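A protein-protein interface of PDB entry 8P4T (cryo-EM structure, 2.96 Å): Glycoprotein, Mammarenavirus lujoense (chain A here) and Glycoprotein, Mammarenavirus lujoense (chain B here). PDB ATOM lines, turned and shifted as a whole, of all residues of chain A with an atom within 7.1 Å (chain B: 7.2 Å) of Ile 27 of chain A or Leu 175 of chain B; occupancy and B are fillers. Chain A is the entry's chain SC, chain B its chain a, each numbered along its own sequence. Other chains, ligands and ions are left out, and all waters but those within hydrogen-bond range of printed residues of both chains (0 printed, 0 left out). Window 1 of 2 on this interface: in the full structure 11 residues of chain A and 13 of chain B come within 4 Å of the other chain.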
ATOM      1  N   ASN A  20       2.482   1.665 -27.958  1.00  0.00           N
ATOM      2  CA  ASN A  20       1.727   1.054 -26.868  1.00  0.00           C
ATOM      3  C   ASN A  20       1.656  -0.460 -27.024  1.00  0.00           C
ATOM      4  O   ASN A  20       1.769  -1.197 -26.038  1.00  0.00           O
ATOM      5  CB  ASN A  20       0.323   1.654 -26.803  1.00  0.00           C
ATOM      6  CG  ASN A  20       0.340   3.146 -26.535  1.00  0.00           C
ATOM      7  OD1 ASN A  20       1.171   3.642 -25.775  1.00  0.00           O
ATOM      8  ND2 ASN A  20      -0.579   3.870 -27.160  1.00  0.00           N
ATOM      9  N   ILE A  21       1.465  -0.942 -28.254  1.00  0.00           N
ATOM     10  CA  ILE A  21       1.436  -2.383 -28.495  1.00  0.00           C
ATOM     11  C   ILE A  21       2.796  -3.002 -28.194  1.00  0.00           C
ATOM     12  O   ILE A  21       2.886  -4.077 -27.588  1.00  0.00           O
ATOM     13  CB  ILE A  21       0.987  -2.672 -29.940  1.00  0.00           C
ATOM     14  CG1 ILE A  21      -0.478  -2.276 -30.132  1.00  0.00           C
ATOM     15  CG2 ILE A  21       1.189  -4.140 -30.284  1.00  0.00           C
ATOM     16  CD1 ILE A  21      -1.412  -2.871 -29.100  1.00  0.00           C
ATOM     17  N   VAL A  22       3.874  -2.334 -28.612  1.00  0.00           N
ATOM     18  CA  VAL A  22       5.219  -2.851 -28.369  1.00  0.00           C
ATOM     19  C   VAL A  22       5.492  -2.957 -26.873  1.00  0.00           C
ATOM     20  O   VAL A  22       6.054  -3.951 -26.398  1.00  0.00           O
ATOM     21  CB  VAL A  22       6.266  -1.969 -29.075  1.00  0.00           C
ATOM     22  CG1 VAL A  22       7.673  -2.430 -28.731  1.00  0.00           C
ATOM     23  CG2 VAL A  22       6.047  -1.988 -30.579  1.00  0.00           C
ATOM     24  N   ILE A  23       5.092  -1.939 -26.110  1.00  0.00           N
ATOM     25  CA  ILE A  23       5.314  -1.949 -24.664  1.00  0.00           C
ATOM     26  C   ILE A  23       4.559  -3.103 -24.014  1.00  0.00           C
ATOM     27  O   ILE A  23       5.100  -3.823 -23.167  1.00  0.00           O
ATOM     28  CB  ILE A  23       4.908  -0.596 -24.054  1.00  0.00           C
ATOM     29  CG1 ILE A  23       5.868   0.506 -24.503  1.00  0.00           C
ATOM     30  CG2 ILE A  23       4.861  -0.691 -22.541  1.00  0.00           C
ATOM     31  CD1 ILE A  23       5.549   1.867 -23.924  1.00  0.00           C
ATOM     32  N   ILE A  24       3.298  -3.296 -24.404  1.00  0.00           N
ATOM     33  CA  ILE A  24       2.472  -4.324 -23.777  1.00  0.00           C
ATOM     34  C   ILE A  24       3.024  -5.713 -24.074  1.00  0.00           C
ATOM     35  O   ILE A  24       3.019  -6.596 -23.206  1.00  0.00           O
ATOM     36  CB  ILE A  24       1.009  -4.178 -24.232  1.00  0.00           C
ATOM     37  CG1 ILE A  24       0.394  -2.912 -23.631  1.00  0.00           C
ATOM     38  CG2 ILE A  24       0.192  -5.400 -23.839  1.00  0.00           C
ATOM     39  CD1 ILE A  24      -1.051  -2.694 -24.011  1.00  0.00           C
ATOM     40  N   VAL A  25       3.517  -5.929 -25.296  1.00  0.00           N
ATOM     41  CA  VAL A  25       4.079  -7.229 -25.654  1.00  0.00           C
ATOM     42  C   VAL A  25       5.307  -7.531 -24.804  1.00  0.00           C
ATOM     43  O   VAL A  25       5.531  -8.678 -24.394  1.00  0.00           O
ATOM     44  CB  VAL A  25       4.399  -7.270 -27.161  1.00  0.00           C
ATOM     45  CG1 VAL A  25       5.319  -8.438 -27.490  1.00  0.00           C
ATOM     46  CG2 VAL A  25       3.115  -7.352 -27.973  1.00  0.00           C
ATOM     47  N   ILE A  26       6.112  -6.508 -24.509  1.00  0.00           N
ATOM     48  CA  ILE A  26       7.293  -6.711 -23.676  1.00  0.00           C
ATOM     49  C   ILE A  26       6.891  -7.080 -22.253  1.00  0.00           C
ATOM     50  O   ILE A  26       7.505  -7.952 -21.625  1.00  0.00           O
ATOM     51  CB  ILE A  26       8.188  -5.458 -23.708  1.00  0.00           C
ATOM     52  CG1 ILE A  26       8.755  -5.242 -25.112  1.00  0.00           C
ATOM     53  CG2 ILE A  26       9.313  -5.572 -22.692  1.00  0.00           C
ATOM     54  CD1 ILE A  26       9.169  -3.812 -25.389  1.00  0.00           C
ATOM     55  N   ILE A  27       5.854  -6.426 -21.723  1.00  0.00           N
ATOM     56  CA  ILE A  27       5.390  -6.728 -20.370  1.00  0.00           C
ATOM     57  C   ILE A  27       4.901  -8.168 -20.279  1.00  0.00           C
ATOM     58  O   ILE A  27       5.179  -8.874 -19.303  1.00  0.00           O
ATOM     59  CB  ILE A  27       4.296  -5.729 -19.947  1.00  0.00           C
ATOM     60  CG1 ILE A  27       4.852  -4.303 -19.941  1.00  0.00           C
ATOM     61  CG2 ILE A  27       3.741  -6.088 -18.578  1.00  0.00           C
ATOM     62  CD1 ILE A  27       3.785  -3.233 -19.935  1.00  0.00           C
ATOM     63  N   MET A  28       4.161  -8.623 -21.294  1.00  0.00           N
ATOM     64  CA  MET A  28       3.621  -9.980 -21.273  1.00  0.00           C
ATOM     65  C   MET A  28       4.732 -11.021 -21.276  1.00  0.00           C
ATOM     66  O   MET A  28       4.651 -12.029 -20.563  1.00  0.00           O
ATOM     67  CB  MET A  28       2.685 -10.188 -22.463  1.00  0.00           C
ATOM     68  CG  MET A  28       1.358  -9.457 -22.344  1.00  0.00           C
ATOM     69  SD  MET A  28       0.390  -9.991 -20.920  1.00  0.00           S
ATOM     70  CE  MET A  28      -0.017 -11.668 -21.398  1.00  0.00           C
ATOM     71  N   PHE A  29       5.778 -10.799 -22.075  1.00  0.00           N
ATOM     72  CA  PHE A  29       6.897 -11.735 -22.115  1.00  0.00           C
ATOM     73  C   PHE A  29       7.635 -11.793 -20.784  1.00  0.00           C
ATOM     74  O   PHE A  29       8.170 -12.846 -20.417  1.00  0.00           O
ATOM     75  CB  PHE A  29       7.860 -11.357 -23.240  1.00  0.00           C
ATOM     76  CG  PHE A  29       7.528 -11.991 -24.560  1.00  0.00           C
ATOM     77  CD1 PHE A  29       7.727 -13.347 -24.762  1.00  0.00           C
ATOM     78  CD2 PHE A  29       7.017 -11.232 -25.600  1.00  0.00           C
ATOM     79  CE1 PHE A  29       7.423 -13.934 -25.976  1.00  0.00           C
ATOM     80  CE2 PHE A  29       6.710 -11.814 -26.817  1.00  0.00           C
ATOM     81  CZ  PHE A  29       6.915 -13.166 -27.005  1.00  0.00           C
ATOM     82  N   THR A  30       7.684 -10.677 -20.052  1.00  0.00           N
ATOM     83  CA  THR A  30       8.308 -10.684 -18.732  1.00  0.00           C
ATOM     84  C   THR A  30       7.554 -11.595 -17.772  1.00  0.00           C
ATOM     85  O   THR A  30       8.168 -12.354 -17.012  1.00  0.00           O
ATOM     86  CB  THR A  30       8.382  -9.262 -18.176  1.00  0.00           C
ATOM     87  OG1 THR A  30       8.792  -8.362 -19.213  1.00  0.00           O
ATOM     88  CG2 THR A  30       9.378  -9.193 -17.030  1.00  0.00           C
ATOM     89  N   LEU A  31       6.220 -11.527 -17.783  1.00  0.00           N
ATOM     90  CA  LEU A  31       5.422 -12.437 -16.968  1.00  0.00           C
ATOM     91  C   LEU A  31       5.648 -13.891 -17.362  1.00  0.00           C
ATOM     92  O   LEU A  31       5.615 -14.779 -16.502  1.00  0.00           O
ATOM     93  CB  LEU A  31       3.939 -12.081 -17.082  1.00  0.00           C
ATOM     94  CG  LEU A  31       3.464 -10.871 -16.276  1.00  0.00           C
ATOM     95  CD1 LEU A  31       2.107 -10.396 -16.773  1.00  0.00           C
ATOM     96  CD2 LEU A  31       3.408 -11.204 -14.794  1.00  0.00           C
ATOM     97  N   ILE A  32       5.871 -14.154 -18.652  1.00  0.00           N
ATOM     98  CA  ILE A  32       6.087 -15.524 -19.108  1.00  0.00           C
ATOM     99  C   ILE A  32       7.382 -16.084 -18.532  1.00  0.00           C
ATOM    100  O   ILE A  32       7.444 -17.251 -18.126  1.00  0.00           O
ATOM    101  CB  ILE A  32       6.078 -15.577 -20.648  1.00  0.00           C
ATOM    102  CG1 ILE A  32       4.688 -15.229 -21.183  1.00  0.00           C
ATOM    103  CG2 ILE A  32       6.508 -16.949 -21.143  1.00  0.00           C
ATOM    104  CD1 ILE A  32       3.601 -16.178 -20.727  1.00  0.00           C
ATOM    105  N   THR B 167       1.031   7.793 -24.723  1.00  0.00           N
ATOM    106  CA  THR B 167       1.502   6.586 -24.048  1.00  0.00           C
ATOM    107  C   THR B 167       0.980   6.567 -22.617  1.00  0.00           C
ATOM    108  O   THR B 167       1.218   7.528 -21.865  1.00  0.00           O
ATOM    109  CB  THR B 167       3.029   6.489 -24.054  1.00  0.00           C
ATOM    110  OG1 THR B 167       3.507   6.533 -25.404  1.00  0.00           O
ATOM    111  CG2 THR B 167       3.482   5.190 -23.404  1.00  0.00           C
ATOM    112  N   ILE B 169       1.005   6.549 -18.995  1.00  0.00           N
ATOM    113  CA  ILE B 169       2.007   6.613 -17.935  1.00  0.00           C
ATOM    114  C   ILE B 169       1.883   5.418 -16.997  1.00  0.00           C
ATOM    115  O   ILE B 169       2.888   4.927 -16.463  1.00  0.00           O
ATOM    116  CB  ILE B 169       1.904   7.949 -17.176  1.00  0.00           C
ATOM    117  CG1 ILE B 169       3.054   8.080 -16.180  1.00  0.00           C
ATOM    118  CG2 ILE B 169       0.558   8.077 -16.477  1.00  0.00           C
ATOM    119  CD1 ILE B 169       3.368   9.494 -15.821  1.00  0.00           C
ATOM    120  N   THR B 170       0.657   4.934 -16.778  1.00  0.00           N
ATOM    121  CA  THR B 170       0.472   3.731 -15.976  1.00  0.00           C
ATOM    122  C   THR B 170       1.168   2.542 -16.621  1.00  0.00           C
ATOM    123  O   THR B 170       1.708   1.677 -15.926  1.00  0.00           O
ATOM    124  CB  THR B 170      -1.018   3.446 -15.785  1.00  0.00           C
ATOM    125  OG1 THR B 170      -1.625   3.191 -17.057  1.00  0.00           O
ATOM    126  CG2 THR B 170      -1.707   4.634 -15.129  1.00  0.00           C
ATOM    127  N   LEU B 171       1.155   2.479 -17.955  1.00  0.00           N
ATOM    128  CA  LEU B 171       1.900   1.441 -18.659  1.00  0.00           C
ATOM    129  C   LEU B 171       3.396   1.550 -18.377  1.00  0.00           C
ATOM    130  O   LEU B 171       4.078   0.535 -18.212  1.00  0.00           O
ATOM    131  CB  LEU B 171       1.619   1.517 -20.160  1.00  0.00           C
ATOM    132  CG  LEU B 171       1.830   0.236 -20.964  1.00  0.00           C
ATOM    133  CD1 LEU B 171       0.997  -0.897 -20.388  1.00  0.00           C
ATOM    134  CD2 LEU B 171       1.484   0.467 -22.425  1.00  0.00           C
ATOM    135  N   MET B 172       3.930   2.775 -18.341  1.00  0.00           N
ATOM    136  CA  MET B 172       5.345   2.956 -18.018  1.00  0.00           C
ATOM    137  C   MET B 172       5.650   2.508 -16.591  1.00  0.00           C
ATOM    138  O   MET B 172       6.689   1.888 -16.332  1.00  0.00           O
ATOM    139  CB  MET B 172       5.746   4.415 -18.222  1.00  0.00           C
ATOM    140  CG  MET B 172       5.971   4.796 -19.676  1.00  0.00           C
ATOM    141  SD  MET B 172       7.401   3.974 -20.404  1.00  0.00           S
ATOM    142  CE  MET B 172       8.652   5.240 -20.215  1.00  0.00           C
ATOM    143  N   ASP B 173       4.763   2.827 -15.646  1.00  0.00           N
ATOM    144  CA  ASP B 173       4.965   2.368 -14.275  1.00  0.00           C
ATOM    145  C   ASP B 173       4.883   0.848 -14.192  1.00  0.00           C
ATOM    146  O   ASP B 173       5.603   0.219 -13.406  1.00  0.00           O
ATOM    147  CB  ASP B 173       3.943   3.017 -13.344  1.00  0.00           C
ATOM    148  CG  ASP B 173       3.977   4.532 -13.406  1.00  0.00           C
ATOM    149  OD1 ASP B 173       4.877   5.079 -14.077  1.00  0.00           O
ATOM    150  OD2 ASP B 173       3.106   5.173 -12.782  1.00  0.00           O
ATOM    151  N   ILE B 174       4.000   0.243 -14.989  1.00  0.00           N
ATOM    152  CA  ILE B 174       3.925  -1.212 -15.070  1.00  0.00           C
ATOM    153  C   ILE B 174       5.211  -1.781 -15.654  1.00  0.00           C
ATOM    154  O   ILE B 174       5.676  -2.845 -15.241  1.00  0.00           O
ATOM    155  CB  ILE B 174       2.687  -1.636 -15.884  1.00  0.00           C
ATOM    156  CG1 ILE B 174       1.416  -1.434 -15.058  1.00  0.00           C
ATOM    157  CG2 ILE B 174       2.794  -3.086 -16.332  1.00  0.00           C
ATOM    158  CD1 ILE B 174       0.148  -1.465 -15.879  1.00  0.00           C
ATOM    159  N   LEU B 175       5.816  -1.077 -16.614  1.00  0.00           N
ATOM    160  CA  LEU B 175       7.132  -1.472 -17.115  1.00  0.00           C
ATOM    161  C   LEU B 175       8.183  -1.431 -16.015  1.00  0.00           C
ATOM    162  O   LEU B 175       9.031  -2.328 -15.917  1.00  0.00           O
ATOM    163  CB  LEU B 175       7.559  -0.559 -18.265  1.00  0.00           C
ATOM    164  CG  LEU B 175       7.150  -0.880 -19.698  1.00  0.00           C
ATOM    165  CD1 LEU B 175       7.546   0.278 -20.599  1.00  0.00           C
ATOM    166  CD2 LEU B 175       7.800  -2.171 -20.164  1.00  0.00           C
ATOM    167  N   MET B 176       8.155  -0.383 -15.194  1.00  0.00           N
ATOM    168  CA  MET B 176       9.112  -0.275 -14.096  1.00  0.00           C
ATOM    169  C   MET B 176       8.934  -1.418 -13.102  1.00  0.00           C
ATOM    170  O   MET B 176       9.906  -2.068 -12.698  1.00  0.00           O
ATOM    171  CB  MET B 176       8.960   1.079 -13.402  1.00  0.00           C
ATOM    172  CG  MET B 176      10.071   1.399 -12.416  1.00  0.00           C
ATOM    173  SD  MET B 176       9.662   2.788 -11.343  1.00  0.00           S
ATOM    174  CE  MET B 176       8.989   3.948 -12.532  1.00  0.00           C
ATOM    175  N   PHE B 177       7.687  -1.691 -12.713  1.00  0.00           N
ATOM    176  CA  PHE B 177       7.410  -2.814 -11.821  1.00  0.00           C
ATOM    177  C   PHE B 177       7.747  -4.152 -12.474  1.00  0.00           C
ATOM    178  O   PHE B 177       8.123  -5.105 -11.782  1.00  0.00           O
ATOM    179  CB  PHE B 177       5.944  -2.783 -11.386  1.00  0.00           C
ATOM    180  CG  PHE B 177       5.457  -4.073 -10.793  1.00  0.00           C
ATOM    181  CD1 PHE B 177       5.923  -4.505  -9.562  1.00  0.00           C
ATOM    182  CD2 PHE B 177       4.531  -4.854 -11.465  1.00  0.00           C
ATOM    183  CE1 PHE B 177       5.476  -5.692  -9.013  1.00  0.00           C
ATOM    184  CE2 PHE B 177       4.080  -6.042 -10.922  1.00  0.00           C
ATOM    185  CZ  PHE B 177       4.553  -6.462  -9.694  1.00  0.00           C
ATOM    186  N   SER B 178       7.625  -4.240 -13.798  1.00  0.00           N
ATOM    187  CA  SER B 178       7.970  -5.466 -14.506  1.00  0.00           C
ATOM    188  C   SER B 178       9.468  -5.718 -14.460  1.00  0.00           C
ATOM    189  O   SER B 178       9.909  -6.841 -14.199  1.00  0.00           O
ATOM    190  CB  SER B 178       7.477  -5.393 -15.951  1.00  0.00           C
ATOM    191  OG  SER B 178       6.122  -4.981 -16.009  1.00  0.00           O
ATOM    192  N   VAL B 179      10.265  -4.679 -14.714  1.00  0.00           N
ATOM    193  CA  VAL B 179      11.711  -4.791 -14.535  1.00  0.00           C
ATOM    194  C   VAL B 179      12.038  -5.151 -13.091  1.00  0.00           C
ATOM    195  O   VAL B 179      12.926  -5.972 -12.824  1.00  0.00           O
ATOM    196  CB  VAL B 179      12.405  -3.486 -14.969  1.00  0.00           C
ATOM    197  CG1 VAL B 179      13.899  -3.555 -14.689  1.00  0.00           C
ATOM    198  CG2 VAL B 179      12.148  -3.215 -16.444  1.00  0.00           C
ATOM    199  N   SER B 180      11.305  -4.566 -12.140  1.00  0.00           N
ATOM    200  CA  SER B 180      11.540  -4.848 -10.727  1.00  0.00           C
ATOM    201  C   SER B 180      11.337  -6.326 -10.409  1.00  0.00           C
ATOM    202  O   SER B 180      12.220  -6.978  -9.838  1.00  0.00           O
ATOM    203  CB  SER B 180      10.624  -3.980  -9.864  1.00  0.00           C
ATOM    204  OG  SER B 180       9.354  -4.587  -9.698  1.00  0.00           O
ATOM    205  N   PHE B 181      10.179  -6.880 -10.769  1.00  0.00           N
ATOM    206  CA  PHE B 181       9.943  -8.273 -10.408  1.00  0.00           C
ATOM    207  C   PHE B 181      10.668  -9.241 -11.335  1.00  0.00           C
ATOM    208  O   PHE B 181      10.858 -10.398 -10.960  1.00  0.00           O
ATOM    209  CB  PHE B 181       8.435  -8.578 -10.342  1.00  0.00           C
ATOM    210  CG  PHE B 181       7.798  -8.955 -11.659  1.00  0.00           C
ATOM    211  CD1 PHE B 181       7.886 -10.251 -12.151  1.00  0.00           C
ATOM    212  CD2 PHE B 181       7.059  -8.029 -12.373  1.00  0.00           C
ATOM    213  CE1 PHE B 181       7.289 -10.598 -13.347  1.00  0.00           C
ATOM    214  CE2 PHE B 181       6.456  -8.375 -13.569  1.00  0.00           C
ATOM    215  CZ  PHE B 181       6.572  -9.659 -14.055  1.00  0.00           C
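CA of Thr 167 of chain B touches OD1 of Asn 20 of chain A, at 3.4 Å. CD1 of Ile 23 of chain A touches CG2 of Thr 167 of chain B, 3.9 Å away. CG2 of Ile 23 of chain A touches CD1 of Leu 175 of chain B, 3.5 Å away. Leu 171 of chain B touches Ile 24 of chain A. Leu 171 of chain B touches Ile 27 of chain A. CD1 of Ile 27 of chain A touches CG2 of Ile 174 of chain B (3.7 Å). CG1 of Ile 27 of chain A touches CD2 of Leu 175 of chain B, at 3.6 Å. Ile 27 of chain A touches Ser 178 of chain B (CG2 to OG, 3.7 Å). CG2 of Thr 30 of chain A touches O of Ser 178 of chain B, 3.7 Å away. Phe 181 of chain B touches Leu 31 of chain A.
Of the printed residues of chain B, Ile 23 of chain A touches Thr 167, Leu 171 and Leu 175. Of the printed residues of chain A, Ile 174 of chain B touches Ile 27. Of chain A, only Ile 23 (3.5 Å) and Ile 27 (3.6 Å) come within 4 Å of Leu 175 of chain B. Printed residues of chain A within 4 Å of Phe 181 of chain B: Leu 31 (3.6 Å). The nearest residue of chain B that does not touch Ile 27 of chain A is Phe 181 of chain B (5.5 Å). The nearest printed residue of chain B that does not touch Ile 23 of chain A is Met 172 of chain B (4.5 Å).
Along chain B the printed residues that touch a printed residue of chain A span positions 167 to 181. Of the 13 printed residues of chain A, 6 touch a printed residue of chain B. Along chain A the printed residues that touch a printed residue of chain B span positions 20 to 31. Among the printed residues, no Asp or Glu carboxylate lies within 4 Å of a Lys or Arg side-chain nitrogen of the other chain.
The side-chain hydroxyl (OG1) of Thr 30 of chain A sits at hydrogen-bond distance from the backbone carbonyl oxygen (O) of Ile 26 of chain A (2.8 Å).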
